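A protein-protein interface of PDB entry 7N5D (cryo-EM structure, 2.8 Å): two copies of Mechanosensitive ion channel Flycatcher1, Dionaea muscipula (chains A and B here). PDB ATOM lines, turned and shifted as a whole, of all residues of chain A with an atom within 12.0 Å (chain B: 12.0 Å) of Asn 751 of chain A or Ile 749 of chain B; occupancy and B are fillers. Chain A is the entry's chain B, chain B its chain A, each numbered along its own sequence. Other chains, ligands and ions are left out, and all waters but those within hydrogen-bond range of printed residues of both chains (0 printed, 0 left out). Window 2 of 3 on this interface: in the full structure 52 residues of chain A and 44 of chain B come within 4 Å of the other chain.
The backbone carbonyl oxygen (O) of Gln 745 of chain B sits at hydrogen-bond distance from the backbone NH (N) of Ser 748 of chain A. The side-chain carboxylate of Glu 746 of chain B lies within salt-bridge range of the guanidinium group of Arg 750 of chain A (3.0 Å). O of Ser 748 of chain A is in hydrogen-bond range of N of Ile 747 of chain B (2.9 Å). The backbone carbonyl oxygen of Ile 747 of chain B is in hydrogen-bond range of the backbone NH of Arg 750 of chain A (2.8 Å). O of Asn 751 of chain A sits at hydrogen-bond distance from N of Ile 749 of chain B (3.1 Å).
Among the printed residues, merely in contact across the chains: Ile 747 of chain A with Gln 745 of chain B, Ile 747 of chain A with Ile 747 of chain B, Ser 748 of chain A with Glu 746 of chain B, Ile 749 of chain A with Ile 747 of chain B, Asn 751 of chain A with Ile 747 of chain B and Asn 751 of chain A with Ser 748 of chain B.
Of chain B, only Ile 747, Ser 748 and Ile 749 come within 4 Å of Asn 751 of chain A. Ile 749 of chain B touches just one residue of chain A: Asn 751. Ile 749 of chain A touches just one residue of chain B: Ile 747. Ser 748 of chain B touches just one residue of chain A: Asn 751. Arg 750 of chain B touches none of the printed residues of chain A. No residue of chain A comes within 4 Å of Asn 751 of chain B. Of the printed residues of chain B, Ile 747 of chain A touches Gln 745 and Ile 747. Of the printed residues of chain A, Gln 745 of chain B touches Ile 747 and Ser 748. The nearest residue of chain B that does not touch Asn 751 of chain A is Arg 750 of chain B (5.3 Å).
Printed residues of chain B that touch a printed residue of chain A: Gln 745, Glu 746, Ile 747, Ser 748 and Ile 749. Hydrophobic or aromatic side chains of chain B within 4 Å of the printed part of chain A: Ile 747. Printed residues of chain A that touch a printed residue of chain B: Ile 747, Ser 748, Ile 749, Arg 750 and Asn 751. Hydrophobic or aromatic side chains of chain A within 4 Å of the printed part of chain B: Ile 747 and Ile 749. Along chain A the printed residues that touch a printed residue of chain B span positions 747 to 751. Among the printed residues, 11 pairs touch across the chains. Among the printed residues, Asp or Glu carboxylates within 4 Å of a Lys or Arg side-chain nitrogen of the other chain: Arg 750 of chain A with Glu 746 of chain B.
Ile 747 of chain A touches its own counterpart, Ile 747 of chain B. Ser 748 of chain A touches Ile 747 of chain B, but with the chains exchanged Ile 747 of chain A does not touch Ser 748 of chain B (7.5 Å). Ile 749 of chain A touches Ile 747 of chain B, but with the chains exchanged Ile 747 of chain A does not touch Ile 749 of chain B (7.5 Å). Asn 751 of chain A touches Ile 749 of chain B, but with the chains exchanged Ile 749 of chain A does not touch Asn 751 of chain B (9.9 Å).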
ATOM      1  N   ILE A 747       1.604  37.748 -23.893  1.00  0.00           N
ATOM      2  CA  ILE A 747       1.706  36.310 -23.827  1.00  0.00           C
ATOM      3  C   ILE A 747       1.789  35.758 -22.427  1.00  0.00           C
ATOM      4  O   ILE A 747       2.472  36.286 -21.541  1.00  0.00           O
ATOM      5  CB  ILE A 747       2.925  35.844 -24.632  1.00  0.00           C
ATOM      6  CG1 ILE A 747       2.803  36.272 -26.100  1.00  0.00           C
ATOM      7  CG2 ILE A 747       3.163  34.382 -24.490  1.00  0.00           C
ATOM      8  CD1 ILE A 747       1.659  35.717 -26.876  1.00  0.00           C
ATOM      9  N   SER A 748       1.058  34.701 -22.214  1.00  0.00           N
ATOM     10  CA  SER A 748       1.111  34.044 -20.941  1.00  0.00           C
ATOM     11  C   SER A 748       1.452  32.611 -21.172  1.00  0.00           C
ATOM     12  O   SER A 748       0.670  31.870 -21.756  1.00  0.00           O
ATOM     13  CB  SER A 748      -0.201  34.161 -20.245  1.00  0.00           C
ATOM     14  OG  SER A 748      -0.166  33.488 -19.034  1.00  0.00           O
ATOM     15  N   ILE A 749       2.622  32.189 -20.739  1.00  0.00           N
ATOM     16  CA  ILE A 749       3.001  30.835 -21.016  1.00  0.00           C
ATOM     17  C   ILE A 749       2.610  29.942 -19.877  1.00  0.00           C
ATOM     18  O   ILE A 749       3.063  30.090 -18.748  1.00  0.00           O
ATOM     19  CB  ILE A 749       4.507  30.718 -21.266  1.00  0.00           C
ATOM     20  CG1 ILE A 749       4.865  31.600 -22.444  1.00  0.00           C
ATOM     21  CG2 ILE A 749       4.867  29.269 -21.547  1.00  0.00           C
ATOM     22  CD1 ILE A 749       6.321  31.810 -22.661  1.00  0.00           C
ATOM     23  N   ARG A 750       1.763  29.002 -20.217  1.00  0.00           N
ATOM     24  CA  ARG A 750       1.234  27.987 -19.323  1.00  0.00           C
ATOM     25  C   ARG A 750       2.280  26.917 -18.960  1.00  0.00           C
ATOM     26  O   ARG A 750       2.246  26.376 -17.856  1.00  0.00           O
ATOM     27  CB  ARG A 750       0.027  27.333 -19.976  1.00  0.00           C
ATOM     28  CG  ARG A 750      -0.662  26.198 -19.217  1.00  0.00           C
ATOM     29  CD  ARG A 750      -1.283  26.629 -17.932  1.00  0.00           C
ATOM     30  NE  ARG A 750      -2.392  27.572 -18.141  1.00  0.00           N
ATOM     31  CZ  ARG A 750      -3.039  28.248 -17.163  1.00  0.00           C
ATOM     32  NH1 ARG A 750      -2.702  28.083 -15.893  1.00  0.00           N
ATOM     33  NH2 ARG A 750      -4.019  29.084 -17.484  1.00  0.00           N
ATOM     34  N   ASN A 751       3.182  26.589 -19.928  1.00  0.00           N
ATOM     35  CA  ASN A 751       4.265  25.601 -19.909  1.00  0.00           C
ATOM     36  C   ASN A 751       3.677  24.238 -20.212  1.00  0.00           C
ATOM     37  O   ASN A 751       3.445  23.906 -21.380  1.00  0.00           O
ATOM     38  CB  ASN A 751       5.098  25.606 -18.588  1.00  0.00           C
ATOM     39  CG  ASN A 751       5.918  26.960 -18.347  1.00  0.00           C
ATOM     40  OD1 ASN A 751       6.613  27.436 -19.268  1.00  0.00           O
ATOM     41  ND2 ASN A 751       5.820  27.550 -17.126  1.00  0.00           N
ATOM     42  N   GLN B 745      -2.832  36.123 -25.178  1.00  0.00           N
ATOM     43  CA  GLN B 745      -2.825  34.785 -25.731  1.00  0.00           C
ATOM     44  C   GLN B 745      -2.070  33.816 -24.866  1.00  0.00           C
ATOM     45  O   GLN B 745      -0.884  34.009 -24.596  1.00  0.00           O
ATOM     46  CB  GLN B 745      -2.230  34.822 -27.126  1.00  0.00           C
ATOM     47  CG  GLN B 745      -2.073  33.508 -27.794  1.00  0.00           C
ATOM     48  CD  GLN B 745      -3.348  32.897 -28.187  1.00  0.00           C
ATOM     49  OE1 GLN B 745      -4.086  33.450 -28.996  1.00  0.00           O
ATOM     50  NE2 GLN B 745      -3.634  31.749 -27.627  1.00  0.00           N
ATOM     51  N   GLU B 746      -2.751  32.768 -24.444  1.00  0.00           N
ATOM     52  CA  GLU B 746      -2.120  31.736 -23.651  1.00  0.00           C
ATOM     53  C   GLU B 746      -1.393  30.769 -24.548  1.00  0.00           C
ATOM     54  O   GLU B 746      -1.942  30.352 -25.572  1.00  0.00           O
ATOM     55  CB  GLU B 746      -3.112  30.991 -22.800  1.00  0.00           C
ATOM     56  CG  GLU B 746      -2.464  29.937 -21.982  1.00  0.00           C
ATOM     57  CD  GLU B 746      -3.359  29.289 -21.046  1.00  0.00           C
ATOM     58  OE1 GLU B 746      -4.068  29.967 -20.356  1.00  0.00           O
ATOM     59  OE2 GLU B 746      -3.361  28.088 -20.993  1.00  0.00           O
ATOM     60  N   ILE B 747      -0.166  30.453 -24.175  1.00  0.00           N
ATOM     61  CA  ILE B 747       0.715  29.569 -24.906  1.00  0.00           C
ATOM     62  C   ILE B 747       1.132  28.349 -24.123  1.00  0.00           C
ATOM     63  O   ILE B 747       1.492  28.428 -22.954  1.00  0.00           O
ATOM     64  CB  ILE B 747       1.963  30.329 -25.348  1.00  0.00           C
ATOM     65  CG1 ILE B 747       1.609  31.511 -26.208  1.00  0.00           C
ATOM     66  CG2 ILE B 747       2.924  29.449 -26.001  1.00  0.00           C
ATOM     67  CD1 ILE B 747       0.933  31.242 -27.492  1.00  0.00           C
ATOM     68  N   SER B 748       1.075  27.212 -24.770  1.00  0.00           N
ATOM     69  CA  SER B 748       1.506  25.947 -24.190  1.00  0.00           C
ATOM     70  C   SER B 748       2.718  25.486 -24.965  1.00  0.00           C
ATOM     71  O   SER B 748       2.731  25.620 -26.184  1.00  0.00           O
ATOM     72  CB  SER B 748       0.400  24.941 -24.276  1.00  0.00           C
ATOM     73  OG  SER B 748       0.831  23.699 -23.849  1.00  0.00           O
ATOM     74  N   ILE B 749       3.781  25.043 -24.298  1.00  0.00           N
ATOM     75  CA  ILE B 749       4.967  24.651 -25.059  1.00  0.00           C
ATOM     76  C   ILE B 749       5.247  23.176 -24.969  1.00  0.00           C
ATOM     77  O   ILE B 749       5.467  22.631 -23.889  1.00  0.00           O
ATOM     78  CB  ILE B 749       6.242  25.380 -24.588  1.00  0.00           C
ATOM     79  CG1 ILE B 749       6.086  26.903 -24.623  1.00  0.00           C
ATOM     80  CG2 ILE B 749       7.441  24.937 -25.444  1.00  0.00           C
ATOM     81  CD1 ILE B 749       5.815  27.513 -25.968  1.00  0.00           C
ATOM     82  N   ARG B 750       5.326  22.536 -26.112  1.00  0.00           N
ATOM     83  CA  ARG B 750       5.633  21.131 -26.143  1.00  0.00           C
ATOM     84  C   ARG B 750       7.089  20.975 -26.570  1.00  0.00           C
ATOM     85  O   ARG B 750       7.413  21.164 -27.745  1.00  0.00           O
ATOM     86  CB  ARG B 750       4.711  20.396 -27.088  1.00  0.00           C
ATOM     87  CG  ARG B 750       4.897  18.898 -27.085  1.00  0.00           C
ATOM     88  CD  ARG B 750       3.938  18.219 -27.977  1.00  0.00           C
ATOM     89  NE  ARG B 750       2.566  18.424 -27.541  1.00  0.00           N
ATOM     90  CZ  ARG B 750       1.911  17.726 -26.580  1.00  0.00           C
ATOM     91  NH1 ARG B 750       2.502  16.736 -25.925  1.00  0.00           N
ATOM     92  NH2 ARG B 750       0.655  18.055 -26.302  1.00  0.00           N
ATOM     93  N   ASN B 751       7.979  20.638 -25.606  1.00  0.00           N
ATOM     94  CA  ASN B 751       9.440  20.508 -25.759  1.00  0.00           C
ATOM     95  C   ASN B 751      10.058  21.788 -26.349  1.00  0.00           C
ATOM     96  O   ASN B 751      10.762  22.531 -25.655  1.00  0.00           O
ATOM     97  CB  ASN B 751       9.825  19.254 -26.604  1.00  0.00           C
ATOM     98  CG  ASN B 751       9.477  17.854 -25.910  1.00  0.00           C
ATOM     99  OD1 ASN B 751       9.442  17.749 -24.666  1.00  0.00           O
ATOM    100  ND2 ASN B 751       9.231  16.801 -26.729  1.00  0.00           N
